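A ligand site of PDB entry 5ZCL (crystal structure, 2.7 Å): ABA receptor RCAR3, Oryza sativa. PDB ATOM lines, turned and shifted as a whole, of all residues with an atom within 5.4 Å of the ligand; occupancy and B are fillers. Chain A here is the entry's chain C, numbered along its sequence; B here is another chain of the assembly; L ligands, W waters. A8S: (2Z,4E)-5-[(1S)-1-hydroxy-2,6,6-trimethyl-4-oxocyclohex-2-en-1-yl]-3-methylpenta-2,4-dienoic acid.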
ATOM      1  N   LYS A  47      16.700 -16.337   8.882  1.00  0.00           N
ATOM      2  CA  LYS A  47      17.376 -17.608   9.121  1.00  0.00           C
ATOM      3  C   LYS A  47      17.116 -18.065  10.552  1.00  0.00           C
ATOM      4  O   LYS A  47      17.585 -17.414  11.487  1.00  0.00           O
ATOM      5  CB  LYS A  47      18.870 -17.469   8.856  1.00  0.00           C
ATOM      6  CG  LYS A  47      19.201 -17.200   7.373  1.00  0.00           C
ATOM      7  CD  LYS A  47      20.697 -17.159   7.106  1.00  0.00           C
ATOM      8  CE  LYS A  47      20.999 -16.818   5.647  1.00  0.00           C
ATOM      9  NZ  LYS A  47      22.457 -16.875   5.356  1.00  0.00           N
ATOM     10  N   PHE A  49      18.372 -20.354  12.270  1.00  0.00           N
ATOM     11  CA  PHE A  49      19.510 -20.953  12.947  1.00  0.00           C
ATOM     12  C   PHE A  49      20.482 -19.922  13.510  1.00  0.00           C
ATOM     13  O   PHE A  49      21.381 -20.307  14.264  1.00  0.00           O
ATOM     14  CB  PHE A  49      20.249 -21.878  11.989  1.00  0.00           C
ATOM     15  CG  PHE A  49      19.489 -23.119  11.663  1.00  0.00           C
ATOM     16  CD1 PHE A  49      19.416 -24.156  12.575  1.00  0.00           C
ATOM     17  CD2 PHE A  49      18.863 -23.255  10.429  1.00  0.00           C
ATOM     18  CE1 PHE A  49      18.712 -25.306  12.275  1.00  0.00           C
ATOM     19  CE2 PHE A  49      18.163 -24.397  10.126  1.00  0.00           C
ATOM     20  CZ  PHE A  49      18.090 -25.431  11.047  1.00  0.00           C
ATOM     21  N   VAL A  69      25.547 -19.419  15.607  1.00  0.00           N
ATOM     22  CA  VAL A  69      24.358 -20.221  15.353  1.00  0.00           C
ATOM     23  C   VAL A  69      23.865 -20.803  16.666  1.00  0.00           C
ATOM     24  O   VAL A  69      24.592 -20.883  17.653  1.00  0.00           O
ATOM     25  CB  VAL A  69      24.616 -21.321  14.313  1.00  0.00           C
ATOM     26  CG1 VAL A  69      24.888 -20.709  12.948  1.00  0.00           C
ATOM     27  CG2 VAL A  69      25.759 -22.200  14.761  1.00  0.00           C
ATOM     28  N   LEU A  73      23.398 -28.006  16.508  1.00  0.00           N
ATOM     29  CA  LEU A  73      24.006 -28.025  15.185  1.00  0.00           C
ATOM     30  C   LEU A  73      25.425 -28.547  15.305  1.00  0.00           C
ATOM     31  O   LEU A  73      25.981 -28.625  16.402  1.00  0.00           O
ATOM     32  CB  LEU A  73      24.015 -26.628  14.535  1.00  0.00           C
ATOM     33  CG  LEU A  73      22.694 -25.971  14.118  1.00  0.00           C
ATOM     34  CD1 LEU A  73      22.944 -24.501  13.869  1.00  0.00           C
ATOM     35  CD2 LEU A  73      22.150 -26.612  12.866  1.00  0.00           C
ATOM     36  N   PRO A  74      26.037 -28.915  14.181  1.00  0.00           N
ATOM     37  CA  PRO A  74      27.429 -29.382  14.203  1.00  0.00           C
ATOM     38  C   PRO A  74      28.456 -28.265  14.328  1.00  0.00           C
ATOM     39  O   PRO A  74      29.654 -28.561  14.379  1.00  0.00           O
ATOM     40  CB  PRO A  74      27.573 -30.100  12.854  1.00  0.00           C
ATOM     41  CG  PRO A  74      26.194 -30.237  12.304  1.00  0.00           C
ATOM     42  CD  PRO A  74      25.414 -29.099  12.869  1.00  0.00           C
ATOM     43  N   ALA A  75      28.045 -26.999  14.337  1.00  0.00           N
ATOM     44  CA  ALA A  75      28.990 -25.891  14.401  1.00  0.00           C
ATOM     45  C   ALA A  75      28.383 -24.777  15.256  1.00  0.00           C
ATOM     46  O   ALA A  75      27.193 -24.805  15.579  1.00  0.00           O
ATOM     47  CB  ALA A  75      29.349 -25.375  12.998  1.00  0.00           C
ATOM     48  N   ARG A  77      29.896 -21.142  14.863  1.00  0.00           N
ATOM     49  CA  ARG A  77      30.205 -19.828  14.320  1.00  0.00           C
ATOM     50  C   ARG A  77      30.760 -19.953  12.911  1.00  0.00           C
ATOM     51  O   ARG A  77      31.479 -20.906  12.594  1.00  0.00           O
ATOM     52  CB  ARG A  77      31.218 -19.131  15.216  1.00  0.00           C
ATOM     53  CG  ARG A  77      32.571 -19.848  15.224  1.00  0.00           C
ATOM     54  CD  ARG A  77      33.613 -19.120  16.031  1.00  0.00           C
ATOM     55  NE  ARG A  77      34.837 -19.907  16.168  1.00  0.00           N
ATOM     56  CZ  ARG A  77      35.859 -19.910  15.320  1.00  0.00           C
ATOM     57  NH1 ARG A  77      35.840 -19.152  14.233  1.00  0.00           N
ATOM     58  NH2 ARG A  77      36.923 -20.667  15.565  1.00  0.00           N
ATOM     59  N   SER A  78      30.428 -18.958  12.067  1.00  0.00           N
ATOM     60  CA  SER A  78      31.052 -18.839  10.750  1.00  0.00           C
ATOM     61  C   SER A  78      31.278 -17.368  10.446  1.00  0.00           C
ATOM     62  O   SER A  78      30.500 -16.508  10.868  1.00  0.00           O
ATOM     63  CB  SER A  78      30.210 -19.456   9.623  1.00  0.00           C
ATOM     64  OG  SER A  78      29.405 -18.481   8.989  1.00  0.00           O
ATOM     65  N   GLU A  80      31.564 -14.703   7.334  1.00  0.00           N
ATOM     66  CA  GLU A  80      31.017 -14.676   5.987  1.00  0.00           C
ATOM     67  C   GLU A  80      31.223 -13.308   5.336  1.00  0.00           C
ATOM     68  O   GLU A  80      31.012 -12.278   5.982  1.00  0.00           O
ATOM     69  CB  GLU A  80      29.540 -15.042   6.021  1.00  0.00           C
ATOM     70  CG  GLU A  80      29.317 -16.305   6.845  1.00  0.00           C
ATOM     71  CD  GLU A  80      27.858 -16.575   7.153  1.00  0.00           C
ATOM     72  OE1 GLU A  80      27.008 -15.725   6.789  1.00  0.00           O
ATOM     73  OE2 GLU A  80      27.568 -17.657   7.729  1.00  0.00           O
ATOM     74  N   PHE A  96      31.685 -18.061   2.741  1.00  0.00           N
ATOM     75  CA  PHE A  96      32.109 -18.389   4.108  1.00  0.00           C
ATOM     76  C   PHE A  96      33.616 -18.490   4.138  1.00  0.00           C
ATOM     77  O   PHE A  96      34.198 -19.323   3.436  1.00  0.00           O
ATOM     78  CB  PHE A  96      31.473 -19.697   4.588  1.00  0.00           C
ATOM     79  CG  PHE A  96      29.979 -19.659   4.649  1.00  0.00           C
ATOM     80  CD1 PHE A  96      29.296 -18.467   4.443  1.00  0.00           C
ATOM     81  CD2 PHE A  96      29.252 -20.803   4.900  1.00  0.00           C
ATOM     82  CE1 PHE A  96      27.905 -18.427   4.491  1.00  0.00           C
ATOM     83  CE2 PHE A  96      27.866 -20.775   4.953  1.00  0.00           C
ATOM     84  CZ  PHE A  96      27.192 -19.583   4.757  1.00  0.00           C
ATOM     85  N   HIS A 101      32.978 -24.694  11.390  1.00  0.00           N
ATOM     86  CA  HIS A 101      32.126 -25.632  10.679  1.00  0.00           C
ATOM     87  C   HIS A 101      32.945 -26.386   9.627  1.00  0.00           C
ATOM     88  O   HIS A 101      34.149 -26.186   9.471  1.00  0.00           O
ATOM     89  CB  HIS A 101      30.933 -24.918  10.041  1.00  0.00           C
ATOM     90  CG  HIS A 101      31.317 -23.848   9.067  1.00  0.00           C
ATOM     91  ND1 HIS A 101      31.730 -24.126   7.779  1.00  0.00           N
ATOM     92  CD2 HIS A 101      31.354 -22.494   9.195  1.00  0.00           C
ATOM     93  CE1 HIS A 101      31.996 -22.994   7.150  1.00  0.00           C
ATOM     94  NE2 HIS A 101      31.776 -21.986   7.990  1.00  0.00           N
ATOM     95  N   LEU A 103      32.078 -26.474   6.251  1.00  0.00           N
ATOM     96  CA  LEU A 103      31.776 -25.985   4.902  1.00  0.00           C
ATOM     97  C   LEU A 103      32.891 -25.051   4.420  1.00  0.00           C
ATOM     98  O   LEU A 103      32.777 -23.825   4.462  1.00  0.00           O
ATOM     99  CB  LEU A 103      30.424 -25.297   4.885  1.00  0.00           C
ATOM    100  CG  LEU A 103      29.246 -26.230   5.152  1.00  0.00           C
ATOM    101  CD1 LEU A 103      27.945 -25.466   5.091  1.00  0.00           C
ATOM    102  CD2 LEU A 103      29.250 -27.344   4.143  1.00  0.00           C
ATOM    103  N   TYR A 106      32.632 -22.325   1.029  1.00  0.00           N
ATOM    104  CA  TYR A 106      31.230 -22.234   0.677  1.00  0.00           C
ATOM    105  C   TYR A 106      30.953 -20.910  -0.035  1.00  0.00           C
ATOM    106  O   TYR A 106      31.420 -19.850   0.393  1.00  0.00           O
ATOM    107  CB  TYR A 106      30.354 -22.352   1.921  1.00  0.00           C
ATOM    108  CG  TYR A 106      28.880 -22.286   1.677  1.00  0.00           C
ATOM    109  CD1 TYR A 106      28.222 -21.056   1.618  1.00  0.00           C
ATOM    110  CD2 TYR A 106      28.126 -23.449   1.514  1.00  0.00           C
ATOM    111  CE1 TYR A 106      26.851 -20.989   1.415  1.00  0.00           C
ATOM    112  CE2 TYR A 106      26.755 -23.386   1.302  1.00  0.00           C
ATOM    113  CZ  TYR A 106      26.119 -22.151   1.251  1.00  0.00           C
ATOM    114  OH  TYR A 106      24.761 -22.087   1.028  1.00  0.00           O
ATOM    115  N   GLU A 127      18.330 -20.110  -4.806  1.00  0.00           N
ATOM    116  CA  GLU A 127      19.612 -20.065  -4.107  1.00  0.00           C
ATOM    117  C   GLU A 127      20.442 -21.280  -4.512  1.00  0.00           C
ATOM    118  O   GLU A 127      19.963 -22.420  -4.407  1.00  0.00           O
ATOM    119  CB  GLU A 127      19.402 -20.042  -2.585  1.00  0.00           C
ATOM    120  CG  GLU A 127      20.693 -19.893  -1.800  1.00  0.00           C
ATOM    121  CD  GLU A 127      20.471 -19.402  -0.376  1.00  0.00           C
ATOM    122  OE1 GLU A 127      19.341 -19.544   0.145  1.00  0.00           O
ATOM    123  OE2 GLU A 127      21.431 -18.863   0.230  1.00  0.00           O
ATOM    124  N   PHE A 145      22.957 -32.087   3.327  1.00  0.00           N
ATOM    125  CA  PHE A 145      23.155 -31.238   4.487  1.00  0.00           C
ATOM    126  C   PHE A 145      22.796 -29.792   4.191  1.00  0.00           C
ATOM    127  O   PHE A 145      22.067 -29.144   4.961  1.00  0.00           O
ATOM    128  CB  PHE A 145      24.618 -31.354   4.936  1.00  0.00           C
ATOM    129  CG  PHE A 145      25.006 -30.443   6.045  1.00  0.00           C
ATOM    130  CD1 PHE A 145      25.510 -29.180   5.781  1.00  0.00           C
ATOM    131  CD2 PHE A 145      24.898 -30.846   7.364  1.00  0.00           C
ATOM    132  CE1 PHE A 145      25.893 -28.340   6.800  1.00  0.00           C
ATOM    133  CE2 PHE A 145      25.286 -30.018   8.389  1.00  0.00           C
ATOM    134  CZ  PHE A 145      25.781 -28.756   8.114  1.00  0.00           C
ATOM    135  N   VAL A 146      23.281 -29.263   3.052  1.00  0.00           N
ATOM    136  CA  VAL A 146      23.061 -27.855   2.749  1.00  0.00           C
ATOM    137  C   VAL A 146      21.610 -27.621   2.337  1.00  0.00           C
ATOM    138  O   VAL A 146      20.974 -26.660   2.769  1.00  0.00           O
ATOM    139  CB  VAL A 146      24.046 -27.395   1.675  1.00  0.00           C
ATOM    140  CG1 VAL A 146      23.755 -25.973   1.237  1.00  0.00           C
ATOM    141  CG2 VAL A 146      25.479 -27.502   2.196  1.00  0.00           C
ATOM    142  N   LEU A 149      19.263 -27.193   5.229  1.00  0.00           N
ATOM    143  CA  LEU A 149      19.350 -25.888   5.864  1.00  0.00           C
ATOM    144  C   LEU A 149      18.746 -24.800   4.974  1.00  0.00           C
ATOM    145  O   LEU A 149      17.971 -23.965   5.450  1.00  0.00           O
ATOM    146  CB  LEU A 149      20.792 -25.557   6.213  1.00  0.00           C
ATOM    147  CG  LEU A 149      21.484 -26.431   7.262  1.00  0.00           C
ATOM    148  CD1 LEU A 149      22.970 -26.114   7.378  1.00  0.00           C
ATOM    149  CD2 LEU A 149      20.810 -26.246   8.615  1.00  0.00           C
ATOM    150  N   LEU A 150      19.087 -24.793   3.676  1.00  0.00           N
ATOM    151  CA  LEU A 150      18.561 -23.756   2.784  1.00  0.00           C
ATOM    152  C   LEU A 150      17.046 -23.852   2.620  1.00  0.00           C
ATOM    153  O   LEU A 150      16.346 -22.837   2.651  1.00  0.00           O
ATOM    154  CB  LEU A 150      19.259 -23.838   1.421  1.00  0.00           C
ATOM    155  CG  LEU A 150      20.761 -23.631   1.355  1.00  0.00           C
ATOM    156  CD1 LEU A 150      21.217 -23.565  -0.089  1.00  0.00           C
ATOM    157  CD2 LEU A 150      21.195 -22.374   2.091  1.00  0.00           C
ATOM    158  N   ASN A 153      15.708 -22.204   5.550  1.00  0.00           N
ATOM    159  CA  ASN A 153      15.833 -20.758   5.464  1.00  0.00           C
ATOM    160  C   ASN A 153      14.761 -20.172   4.553  1.00  0.00           C
ATOM    161  O   ASN A 153      14.018 -19.266   4.955  1.00  0.00           O
ATOM    162  CB  ASN A 153      17.227 -20.378   4.970  1.00  0.00           C
ATOM    163  CG  ASN A 153      18.294 -20.530   6.047  1.00  0.00           C
ATOM    164  OD1 ASN A 153      17.981 -20.697   7.227  1.00  0.00           O
ATOM    165  ND2 ASN A 153      19.554 -20.478   5.638  1.00  0.00           N
ATOM    166  N   TRP B 202      29.032 -36.181  10.550  1.00  0.00           N
ATOM    167  CA  TRP B 202      29.306 -34.757  10.362  1.00  0.00           C
ATOM    168  C   TRP B 202      29.551 -34.167  11.759  1.00  0.00           C
ATOM    169  O   TRP B 202      28.669 -33.592  12.400  1.00  0.00           O
ATOM    170  CB  TRP B 202      28.143 -34.073   9.661  1.00  0.00           C
ATOM    171  CG  TRP B 202      28.491 -32.780   9.028  1.00  0.00           C
ATOM    172  CD1 TRP B 202      28.713 -31.598   9.647  1.00  0.00           C
ATOM    173  CD2 TRP B 202      28.640 -32.541   7.625  1.00  0.00           C
ATOM    174  NE1 TRP B 202      28.993 -30.622   8.725  1.00  0.00           N
ATOM    175  CE2 TRP B 202      28.962 -31.171   7.481  1.00  0.00           C
ATOM    176  CE3 TRP B 202      28.540 -33.336   6.485  1.00  0.00           C
ATOM    177  CZ2 TRP B 202      29.179 -30.588   6.237  1.00  0.00           C
ATOM    178  CZ3 TRP B 202      28.753 -32.757   5.253  1.00  0.00           C
ATOM    179  CH2 TRP B 202      29.067 -31.396   5.135  1.00  0.00           C
HETATM  180  C1  A8S L   1      22.992 -20.274   5.131  1.00  0.00           C
HETATM  181  C2  A8S L   1      23.487 -21.632   4.640  1.00  0.00           C
HETATM  182  C3  A8S L   1      24.102 -22.566   5.400  1.00  0.00           C
HETATM  183  C4  A8S L   1      24.351 -22.360   6.828  1.00  0.00           C
HETATM  184  C5  A8S L   1      25.255 -23.058   7.529  1.00  0.00           C
HETATM  185  C6  A8S L   1      24.556 -23.844   4.768  1.00  0.00           C
HETATM  186  C7  A8S L   1      25.481 -22.812   8.994  1.00  0.00           C
HETATM  187  O7  A8S L   1      25.055 -21.554   9.472  1.00  0.00           O
HETATM  188  C8  A8S L   1      24.711 -23.831   9.768  1.00  0.00           C
HETATM  189  C9  A8S L   1      25.279 -24.904  10.316  1.00  0.00           C
HETATM  190  C10 A8S L   1      26.640 -25.305   9.975  1.00  0.00           C
HETATM  191  O10 A8S L   1      27.068 -26.403  10.298  1.00  0.00           O
HETATM  192  C11 A8S L   1      27.491 -24.321   9.215  1.00  0.00           C
HETATM  193  O11 A8S L   1      22.511 -19.485   4.245  1.00  0.00           O
HETATM  194  C12 A8S L   1      27.007 -22.866   9.297  1.00  0.00           C
HETATM  195  O12 A8S L   1      23.064 -20.000   6.338  1.00  0.00           O
HETATM  196  C13 A8S L   1      23.236 -23.662   9.795  1.00  0.00           C
HETATM  197  C14 A8S L   1      27.324 -22.347  10.669  1.00  0.00           C
HETATM  198  C15 A8S L   1      27.788 -22.045   8.270  1.00  0.00           C
HETATM  199  O   HOH W   1      19.397 -19.089   2.718  1.00  0.00           O
HETATM  200  O   HOH W   2      23.690 -19.740   1.863  1.00  0.00           O
HETATM  201  O   HOH W   3      25.608 -19.453   8.055  1.00  0.00           O
HETATM  202  O   HOH W   4      22.484 -20.230   8.828  1.00  0.00           O
HETATM  203  O   HOH W   5      29.672 -27.740   9.852  1.00  0.00           O
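Residues that only touch the ligand: Leu 149, Phe 145, Leu 150, Phe 96, Val 69, His 101, Ala 75, Leu 103, Ser 78 and Tyr 106.
Hydrophobic or aromatic side chains that line the ligand: Val 69, Ala 75, Phe 96, His 101, Leu 103, Phe 145, Leu 149 and Leu 150.
12 residues have an atom within 4 Å of the ligand: Lys 47, Val 69, Ala 75, Ser 78, Phe 96, His 101, Leu 103, Tyr 106, Phe 145, Leu 149, Leu 150 and Asn 153.
The nearest printed residue that does not touch the ligand is Pro 74 (4.1 Å).
An oxygen (O11) of the ligand is in salt-bridge range of the side-chain amino group of Lys 47 (2.8 Å).
An oxygen (O11) of the ligand lies within hydrogen-bond range of the side-chain amide nitrogen (ND2) of Asn 153, 3.4 Å away.
O of Tyr 106 lies within hydrogen-bond range of N of Phe 96 (3.0 Å).
ND1 of His 101 is in hydrogen-bond range of N of Leu 103, at 2.8 Å.
Water W3 lies within hydrogen-bond range of O7 of the ligand (2.6 Å) and OE2 of Glu 80 (2.7 Å).
Water W2 lies within hydrogen-bond range of O11 of the ligand, OH of Tyr 106 and OE2 of Glu 127.
Water W5 lies within hydrogen-bond range of an oxygen (O10) of the ligand (3.0 Å) and the indole nitrogen (NE1) of Trp 202 of chain B (3.2 Å).
Water W1 lies within hydrogen-bond range of OE1 of Glu 127 (2.6 Å), ND2 of Asn 153 (3.2 Å) and O11 of the ligand (3.5 Å).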
